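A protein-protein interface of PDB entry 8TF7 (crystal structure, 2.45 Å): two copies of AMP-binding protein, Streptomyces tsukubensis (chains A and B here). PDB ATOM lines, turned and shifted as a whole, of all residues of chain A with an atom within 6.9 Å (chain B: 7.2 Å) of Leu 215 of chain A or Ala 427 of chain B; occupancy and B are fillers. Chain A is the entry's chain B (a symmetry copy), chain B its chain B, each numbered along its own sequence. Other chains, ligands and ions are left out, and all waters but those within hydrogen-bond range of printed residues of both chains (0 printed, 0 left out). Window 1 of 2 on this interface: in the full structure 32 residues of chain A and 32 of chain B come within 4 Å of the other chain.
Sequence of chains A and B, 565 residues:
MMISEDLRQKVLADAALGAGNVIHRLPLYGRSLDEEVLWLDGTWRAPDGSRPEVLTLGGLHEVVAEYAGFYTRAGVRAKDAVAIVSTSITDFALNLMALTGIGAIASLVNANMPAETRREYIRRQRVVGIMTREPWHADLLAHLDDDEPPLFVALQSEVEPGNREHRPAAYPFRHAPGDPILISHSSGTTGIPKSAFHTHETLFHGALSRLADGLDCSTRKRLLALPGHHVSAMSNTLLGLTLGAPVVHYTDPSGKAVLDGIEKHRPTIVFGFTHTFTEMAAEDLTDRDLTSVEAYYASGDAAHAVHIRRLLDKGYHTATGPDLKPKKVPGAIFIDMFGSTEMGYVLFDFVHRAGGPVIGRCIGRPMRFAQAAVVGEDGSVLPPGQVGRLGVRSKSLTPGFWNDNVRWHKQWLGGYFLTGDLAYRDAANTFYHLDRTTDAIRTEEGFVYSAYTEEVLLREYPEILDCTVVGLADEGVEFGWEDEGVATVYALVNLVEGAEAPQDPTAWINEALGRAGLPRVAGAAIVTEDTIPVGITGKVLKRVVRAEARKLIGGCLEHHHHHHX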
ATOM      1  N   MET A   2     -24.848  -7.473  12.566  1.00  0.00           N
ATOM      2  CA  MET A   2     -26.022  -6.632  12.745  1.00  0.00           C
ATOM      3  C   MET A   2     -27.180  -7.141  11.893  1.00  0.00           C
ATOM      4  O   MET A   2     -26.987  -7.722  10.822  1.00  0.00           O
ATOM      5  CB  MET A   2     -25.686  -5.186  12.377  1.00  0.00           C
ATOM      6  CG  MET A   2     -26.840  -4.211  12.504  1.00  0.00           C
ATOM      7  SD  MET A   2     -26.280  -2.533  12.861  1.00  0.00           S
ATOM      8  CE  MET A   2     -26.460  -1.762  11.254  1.00  0.00           C
ATOM      9  N   ARG A   8     -34.689  -4.271  10.179  1.00  0.00           N
ATOM     10  CA  ARG A   8     -34.670  -3.024  10.935  1.00  0.00           C
ATOM     11  C   ARG A   8     -35.843  -2.133  10.548  1.00  0.00           C
ATOM     12  O   ARG A   8     -36.511  -1.563  11.421  1.00  0.00           O
ATOM     13  CB  ARG A   8     -33.340  -2.302  10.700  1.00  0.00           C
ATOM     14  CG  ARG A   8     -33.340  -0.835  11.090  1.00  0.00           C
ATOM     15  CD  ARG A   8     -32.012  -0.173  10.758  1.00  0.00           C
ATOM     16  NE  ARG A   8     -32.012   1.236  11.128  1.00  0.00           N
ATOM     17  CZ  ARG A   8     -31.756   1.693  12.347  1.00  0.00           C
ATOM     18  NH1 ARG A   8     -31.454   0.875  13.342  1.00  0.00           N
ATOM     19  NH2 ARG A   8     -31.806   3.002  12.572  1.00  0.00           N
ATOM     20  N   GLY A 206     -36.280   0.388  26.039  1.00  0.00           N
ATOM     21  CA  GLY A 206     -34.834   0.501  25.936  1.00  0.00           C
ATOM     22  C   GLY A 206     -34.267  -0.286  24.771  1.00  0.00           C
ATOM     23  O   GLY A 206     -33.333   0.166  24.100  1.00  0.00           O
ATOM     24  N   ALA A 207     -34.822  -1.470  24.507  1.00  0.00           N
ATOM     25  CA  ALA A 207     -34.309  -2.289  23.415  1.00  0.00           C
ATOM     26  C   ALA A 207     -34.630  -1.668  22.062  1.00  0.00           C
ATOM     27  O   ALA A 207     -33.801  -1.703  21.145  1.00  0.00           O
ATOM     28  CB  ALA A 207     -34.883  -3.704  23.504  1.00  0.00           C
ATOM     29  N   LEU A 208     -35.828  -1.099  21.911  1.00  0.00           N
ATOM     30  CA  LEU A 208     -36.180  -0.474  20.641  1.00  0.00           C
ATOM     31  C   LEU A 208     -35.402   0.820  20.435  1.00  0.00           C
ATOM     32  O   LEU A 208     -35.005   1.141  19.310  1.00  0.00           O
ATOM     33  CB  LEU A 208     -37.681  -0.208  20.578  1.00  0.00           C
ATOM     34  CG  LEU A 208     -38.579  -1.437  20.448  1.00  0.00           C
ATOM     35  CD1 LEU A 208     -40.040  -1.012  20.371  1.00  0.00           C
ATOM     36  CD2 LEU A 208     -38.198  -2.274  19.237  1.00  0.00           C
ATOM     37  N   SER A 209     -35.175   1.577  21.510  1.00  0.00           N
ATOM     38  CA  SER A 209     -34.402   2.808  21.391  1.00  0.00           C
ATOM     39  C   SER A 209     -32.975   2.507  20.949  1.00  0.00           C
ATOM     40  O   SER A 209     -32.438   3.164  20.049  1.00  0.00           O
ATOM     41  CB  SER A 209     -34.408   3.560  22.720  1.00  0.00           C
ATOM     42  OG  SER A 209     -33.325   4.474  22.782  1.00  0.00           O
ATOM     43  N   ARG A 210     -32.343   1.511  21.576  1.00  0.00           N
ATOM     44  CA  ARG A 210     -30.990   1.130  21.185  1.00  0.00           C
ATOM     45  C   ARG A 210     -30.962   0.633  19.744  1.00  0.00           C
ATOM     46  O   ARG A 210     -30.086   1.014  18.959  1.00  0.00           O
ATOM     47  CB  ARG A 210     -30.454   0.059  22.135  1.00  0.00           C
ATOM     48  CG  ARG A 210     -30.360   0.504  23.587  1.00  0.00           C
ATOM     49  CD  ARG A 210     -29.059   1.242  23.862  1.00  0.00           C
ATOM     50  NE  ARG A 210     -27.928   0.331  23.991  1.00  0.00           N
ATOM     51  CZ  ARG A 210     -26.689   0.710  24.270  1.00  0.00           C
ATOM     52  NH1 ARG A 210     -26.382   1.983  24.459  1.00  0.00           N
ATOM     53  NH2 ARG A 210     -25.734  -0.211  24.363  1.00  0.00           N
ATOM     54  N   LEU A 211     -31.919  -0.224  19.379  1.00  0.00           N
ATOM     55  CA  LEU A 211     -32.007  -0.703  18.003  1.00  0.00           C
ATOM     56  C   LEU A 211     -32.072   0.463  17.023  1.00  0.00           C
ATOM     57  O   LEU A 211     -31.388   0.464  15.993  1.00  0.00           O
ATOM     58  CB  LEU A 211     -33.230  -1.605  17.844  1.00  0.00           C
ATOM     59  CG  LEU A 211     -33.365  -2.301  16.489  1.00  0.00           C
ATOM     60  CD1 LEU A 211     -33.938  -3.700  16.662  1.00  0.00           C
ATOM     61  CD2 LEU A 211     -34.227  -1.480  15.544  1.00  0.00           C
ATOM     62  N   ALA A 212     -32.897   1.469  17.329  1.00  0.00           N
ATOM     63  CA  ALA A 212     -32.982   2.643  16.470  1.00  0.00           C
ATOM     64  C   ALA A 212     -31.620   3.294  16.275  1.00  0.00           C
ATOM     65  O   ALA A 212     -31.343   3.853  15.207  1.00  0.00           O
ATOM     66  CB  ALA A 212     -33.964   3.656  17.059  1.00  0.00           C
ATOM     67  N   ASP A 213     -30.763   3.240  17.291  1.00  0.00           N
ATOM     68  CA  ASP A 213     -29.432   3.824  17.228  1.00  0.00           C
ATOM     69  C   ASP A 213     -28.402   2.870  16.637  1.00  0.00           C
ATOM     70  O   ASP A 213     -27.203   3.164  16.686  1.00  0.00           O
ATOM     71  CB  ASP A 213     -28.988   4.265  18.625  1.00  0.00           C
ATOM     72  CG  ASP A 213     -29.671   5.541  19.082  1.00  0.00           C
ATOM     73  OD1 ASP A 213     -30.313   6.210  18.245  1.00  0.00           O
ATOM     74  OD2 ASP A 213     -29.566   5.872  20.283  1.00  0.00           O
ATOM     75  N   GLY A 214     -28.837   1.742  16.085  1.00  0.00           N
ATOM     76  CA  GLY A 214     -27.904   0.767  15.558  1.00  0.00           C
ATOM     77  C   GLY A 214     -27.122   0.024  16.616  1.00  0.00           C
ATOM     78  O   GLY A 214     -25.957  -0.320  16.389  1.00  0.00           O
ATOM     79  N   LEU A 215     -27.732  -0.240  17.769  1.00  0.00           N
ATOM     80  CA  LEU A 215     -27.065  -0.909  18.875  1.00  0.00           C
ATOM     81  C   LEU A 215     -27.929  -2.056  19.382  1.00  0.00           C
ATOM     82  O   LEU A 215     -29.143  -2.088  19.172  1.00  0.00           O
ATOM     83  CB  LEU A 215     -26.768   0.070  20.021  1.00  0.00           C
ATOM     84  CG  LEU A 215     -25.910   1.282  19.651  1.00  0.00           C
ATOM     85  CD1 LEU A 215     -26.069   2.396  20.677  1.00  0.00           C
ATOM     86  CD2 LEU A 215     -24.447   0.887  19.513  1.00  0.00           C
ATOM     87  N   ASP A 216     -27.276  -3.003  20.056  1.00  0.00           N
ATOM     88  CA  ASP A 216     -27.942  -4.151  20.669  1.00  0.00           C
ATOM     89  C   ASP A 216     -28.927  -4.803  19.702  1.00  0.00           C
ATOM     90  O   ASP A 216     -30.067  -5.119  20.054  1.00  0.00           O
ATOM     91  CB  ASP A 216     -28.653  -3.741  21.963  1.00  0.00           C
ATOM     92  CG  ASP A 216     -27.699  -3.213  23.015  1.00  0.00           C
ATOM     93  OD1 ASP A 216     -26.477  -3.437  22.885  1.00  0.00           O
ATOM     94  OD2 ASP A 216     -28.176  -2.574  23.979  1.00  0.00           O
ATOM     95  N   CYS A 217     -28.476  -5.013  18.469  1.00  0.00           N
ATOM     96  CA  CYS A 217     -29.334  -5.532  17.410  1.00  0.00           C
ATOM     97  C   CYS A 217     -28.548  -6.446  16.479  1.00  0.00           C
ATOM     98  O   CYS A 217     -28.554  -6.287  15.259  1.00  0.00           O
ATOM     99  CB  CYS A 217     -29.972  -4.384  16.627  1.00  0.00           C
ATOM    100  SG  CYS A 217     -28.785  -3.140  16.061  1.00  0.00           S
ATOM    101  N   SER A 218     -27.867  -7.429  17.054  1.00  0.00           N
ATOM    102  CA  SER A 218     -27.142  -8.428  16.284  1.00  0.00           C
ATOM    103  C   SER A 218     -27.919  -9.740  16.253  1.00  0.00           C
ATOM    104  O   SER A 218     -28.823  -9.977  17.060  1.00  0.00           O
ATOM    105  CB  SER A 218     -25.749  -8.662  16.874  1.00  0.00           C
ATOM    106  OG  SER A 218     -25.837  -9.240  18.163  1.00  0.00           O
ATOM    107  N   LEU A 243     -34.755 -10.201  16.987  1.00  0.00           N
ATOM    108  CA  LEU A 243     -33.628 -10.004  16.086  1.00  0.00           C
ATOM    109  C   LEU A 243     -33.386 -11.199  15.173  1.00  0.00           C
ATOM    110  O   LEU A 243     -32.596 -11.083  14.227  1.00  0.00           O
ATOM    111  CB  LEU A 243     -32.358  -9.718  16.892  1.00  0.00           C
ATOM    112  CG  LEU A 243     -32.374  -8.467  17.774  1.00  0.00           C
ATOM    113  CD1 LEU A 243     -31.157  -8.422  18.693  1.00  0.00           C
ATOM    114  CD2 LEU A 243     -32.449  -7.211  16.915  1.00  0.00           C
ATOM    115  N   THR A 318     -13.656  -8.409  18.150  1.00  0.00           N
ATOM    116  CA  THR A 318     -13.373  -7.849  16.838  1.00  0.00           C
ATOM    117  C   THR A 318     -13.226  -6.337  16.940  1.00  0.00           C
ATOM    118  O   THR A 318     -13.954  -5.680  17.690  1.00  0.00           O
ATOM    119  CB  THR A 318     -14.481  -8.196  15.842  1.00  0.00           C
ATOM    120  OG1 THR A 318     -14.577  -9.620  15.710  1.00  0.00           O
ATOM    121  CG2 THR A 318     -14.194  -7.578  14.481  1.00  0.00           C
ATOM    122  N   ASP A 349     -24.265   2.405  30.407  1.00  0.00           N
ATOM    123  CA  ASP A 349     -23.342   1.754  29.482  1.00  0.00           C
ATOM    124  C   ASP A 349     -21.941   1.774  30.085  1.00  0.00           C
ATOM    125  O   ASP A 349     -21.304   2.831  30.155  1.00  0.00           O
ATOM    126  CB  ASP A 349     -23.358   2.448  28.119  1.00  0.00           C
ATOM    127  CG  ASP A 349     -23.093   1.487  26.971  1.00  0.00           C
ATOM    128  OD1 ASP A 349     -22.954   0.274  27.228  1.00  0.00           O
ATOM    129  OD2 ASP A 349     -23.026   1.945  25.809  1.00  0.00           O
ATOM    130  N   ARG B 365     -18.884  10.196  21.643  1.00  0.00           N
ATOM    131  CA  ARG B 365     -20.214   9.609  21.642  1.00  0.00           C
ATOM    132  C   ARG B 365     -21.268  10.703  21.546  1.00  0.00           C
ATOM    133  O   ARG B 365     -21.026  11.847  21.944  1.00  0.00           O
ATOM    134  CB  ARG B 365     -20.448   8.792  22.915  1.00  0.00           C
ATOM    135  CG  ARG B 365     -20.610   7.296  22.665  1.00  0.00           C
ATOM    136  CD  ARG B 365     -20.467   6.486  23.948  1.00  0.00           C
ATOM    137  NE  ARG B 365     -19.280   5.638  23.926  1.00  0.00           N
ATOM    138  CZ  ARG B 365     -18.730   5.086  24.998  1.00  0.00           C
ATOM    139  NH1 ARG B 365     -19.244   5.257  26.205  1.00  0.00           N
ATOM    140  NH2 ARG B 365     -17.635   4.344  24.856  1.00  0.00           N
ATOM    141  N   VAL B 381     -28.464   2.390   7.831  1.00  0.00           N
ATOM    142  CA  VAL B 381     -27.557   2.538   8.963  1.00  0.00           C
ATOM    143  C   VAL B 381     -26.521   1.425   8.906  1.00  0.00           C
ATOM    144  O   VAL B 381     -26.864   0.238   8.829  1.00  0.00           O
ATOM    145  CB  VAL B 381     -28.327   2.513  10.292  1.00  0.00           C
ATOM    146  CG1 VAL B 381     -27.362   2.390  11.463  1.00  0.00           C
ATOM    147  CG2 VAL B 381     -29.176   3.765  10.437  1.00  0.00           C
ATOM    148  N   PRO B 384     -21.170  -1.332  13.020  1.00  0.00           N
ATOM    149  CA  PRO B 384     -19.871  -0.809  13.452  1.00  0.00           C
ATOM    150  C   PRO B 384     -18.750  -1.392  12.610  1.00  0.00           C
ATOM    151  O   PRO B 384     -18.800  -2.546  12.179  1.00  0.00           O
ATOM    152  CB  PRO B 384     -19.763  -1.258  14.916  1.00  0.00           C
ATOM    153  CG  PRO B 384     -21.125  -1.763  15.295  1.00  0.00           C
ATOM    154  CD  PRO B 384     -21.780  -2.214  14.029  1.00  0.00           C
ATOM    155  N   GLY B 385     -17.732  -0.571  12.367  1.00  0.00           N
ATOM    156  CA  GLY B 385     -16.575  -0.991  11.611  1.00  0.00           C
ATOM    157  C   GLY B 385     -16.622  -0.695  10.128  1.00  0.00           C
ATOM    158  O   GLY B 385     -15.630  -0.951   9.433  1.00  0.00           O
ATOM    159  N   ARG B 425     -17.934   3.927  13.225  1.00  0.00           N
ATOM    160  CA  ARG B 425     -18.165   3.818  14.656  1.00  0.00           C
ATOM    161  C   ARG B 425     -17.795   2.416  15.119  1.00  0.00           C
ATOM    162  O   ARG B 425     -17.726   1.475  14.323  1.00  0.00           O
ATOM    163  CB  ARG B 425     -19.625   4.114  15.021  1.00  0.00           C
ATOM    164  CG  ARG B 425     -20.638   3.373  14.162  1.00  0.00           C
ATOM    165  CD  ARG B 425     -21.921   3.109  14.932  1.00  0.00           C
ATOM    166  NE  ARG B 425     -22.831   2.234  14.203  1.00  0.00           N
ATOM    167  CZ  ARG B 425     -23.606   1.317  14.770  1.00  0.00           C
ATOM    168  NH1 ARG B 425     -23.600   1.119  16.078  1.00  0.00           N
ATOM    169  NH2 ARG B 425     -24.407   0.581  14.003  1.00  0.00           N
ATOM    170  N   ASP B 426     -17.552   2.285  16.420  1.00  0.00           N
ATOM    171  CA  ASP B 426     -17.354   0.989  17.044  1.00  0.00           C
ATOM    172  C   ASP B 426     -18.668   0.550  17.691  1.00  0.00           C
ATOM    173  O   ASP B 426     -19.716   1.178  17.511  1.00  0.00           O
ATOM    174  CB  ASP B 426     -16.196   1.041  18.043  1.00  0.00           C
ATOM    175  CG  ASP B 426     -16.403   2.069  19.139  1.00  0.00           C
ATOM    176  OD1 ASP B 426     -17.556   2.274  19.569  1.00  0.00           O
ATOM    177  OD2 ASP B 426     -15.398   2.667  19.581  1.00  0.00           O
ATOM    178  N   ALA B 427     -18.624  -0.541  18.454  1.00  0.00           N
ATOM    179  CA  ALA B 427     -19.850  -1.105  19.004  1.00  0.00           C
ATOM    180  C   ALA B 427     -20.394  -0.318  20.189  1.00  0.00           C
ATOM    181  O   ALA B 427     -21.522  -0.584  20.620  1.00  0.00           O
ATOM    182  CB  ALA B 427     -19.621  -2.561  19.413  1.00  0.00           C
ATOM    183  N   ALA B 428     -19.635   0.641  20.719  1.00  0.00           N
ATOM    184  CA  ALA B 428     -20.108   1.518  21.782  1.00  0.00           C
ATOM    185  C   ALA B 428     -20.642   2.843  21.251  1.00  0.00           C
ATOM    186  O   ALA B 428     -20.874   3.767  22.038  1.00  0.00           O
ATOM    187  CB  ALA B 428     -18.986   1.779  22.788  1.00  0.00           C
ATOM    188  N   ASN B 429     -20.843   2.953  19.938  1.00  0.00           N
ATOM    189  CA  ASN B 429     -21.292   4.195  19.305  1.00  0.00           C
ATOM    190  C   ASN B 429     -20.323   5.343  19.585  1.00  0.00           C
ATOM    191  O   ASN B 429     -20.725   6.494  19.777  1.00  0.00           O
ATOM    192  CB  ASN B 429     -22.710   4.562  19.738  1.00  0.00           C
ATOM    193  CG  ASN B 429     -23.636   4.775  18.555  1.00  0.00           C
ATOM    194  OD1 ASN B 429     -23.480   4.139  17.510  1.00  0.00           O
ATOM    195  ND2 ASN B 429     -24.599   5.674  18.710  1.00  0.00           N
ATOM    196  N   THR B 430     -19.032   5.028  19.613  1.00  0.00           N
ATOM    197  CA  THR B 430     -17.985   6.038  19.561  1.00  0.00           C
ATOM    198  C   THR B 430     -17.577   6.216  18.102  1.00  0.00           C
ATOM    199  O   THR B 430     -17.269   5.235  17.417  1.00  0.00           O
ATOM    200  CB  THR B 430     -16.786   5.629  20.410  1.00  0.00           C
ATOM    201  OG1 THR B 430     -17.183   5.534  21.783  1.00  0.00           O
ATOM    202  CG2 THR B 430     -15.667   6.652  20.280  1.00  0.00           C
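Of the 18 printed residues of chain A, 5 touch a printed residue of chain B.
Hydrophobic or aromatic side chains of chain A within 4 Å of the printed part of chain B: Met 2 and Leu 215.
Hydrophobic or aromatic side chains of chain B within 4 Å of the printed part of chain A: Val 381.
Along chain B the printed residues that touch a printed residue of chain A span positions 381 to 429.
Among the printed residues, no Asp or Glu carboxylate lies within 4 Å of a Lys or Arg side-chain nitrogen of the other chain.
NH2 of Arg 8 of chain A is in hydrogen-bond range of O of Ala 212 of chain A.
The backbone carbonyl oxygen (O) of Leu 215 of chain A lies within hydrogen-bond range of the side-chain sulfur (SG) of Cys 217 of chain A (3.3 Å).
The side-chain amide oxygen (OD1) of Asn 429 of chain B sits close to the guanidinium group (NH1) of Arg 425 of chain B, at 3.3 Å.
The backbone NH (N) of Asn 429 of chain B sits at hydrogen-bond distance from the side-chain carboxylate (OD1) of Asp 426 of chain B (3.4 Å).
The backbone carbonyl oxygen of Arg 210 of chain A lies within hydrogen-bond range of the backbone NH of Leu 215 of chain A, 2.9 Å away.
NH1 of Arg 8 of chain A lies within hydrogen-bond range of O of Leu 211 of chain A, 2.7 Å away.
Val 381 of chain B touches Met 2 of chain A (O to CE, 3.2 Å).
NH2 of Arg 425 of chain B touches SD of Met 2 of chain A, 3.8 Å away.
Arg 8 of chain A touches Val 381 of chain B (NH2 to CG2, 3.5 Å).
Asn 429 of chain B touches Asp 213 of chain A (OD1 to O, 3.9 Å).
Leu 215 of chain A touches Arg 425 of chain B (CD2 to NH1, 3.5 Å).
O of Ala 427 of chain B touches CD2 of Leu 215 of chain A, at 3.5 Å.
CD2 of Leu 215 of chain A touches OD1 of Asn 429 of chain B (3.9 Å).
No position is printed for both chains.
NH1 of Arg 425 of chain B sits at hydrogen-bond distance from O of Gly 214 of chain A (2.8 Å).
Of the printed residues of chain B, Met 2 of chain A touches Val 381 (3.2 Å) and Arg 425 (3.8 Å).
Ala 207 of chain A touches none of the printed residues of chain B.
Gly 214 of chain A touches one residue of chain B.
Leu 215 of chain A touches just these residues of chain B: Arg 425 (3.5 Å), Ala 427 (3.5 Å) and Asn 429 (3.9 Å).
Of the printed residues of chain A, Arg 425 of chain B touches Met 2, Gly 214 and Leu 215.
Of chain A, only Leu 215 comes within 4 Å of Ala 427 of chain B.
The nearest residue of chain B that does not touch Leu 215 of chain A is Ala 428 of chain B (4.6 Å).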
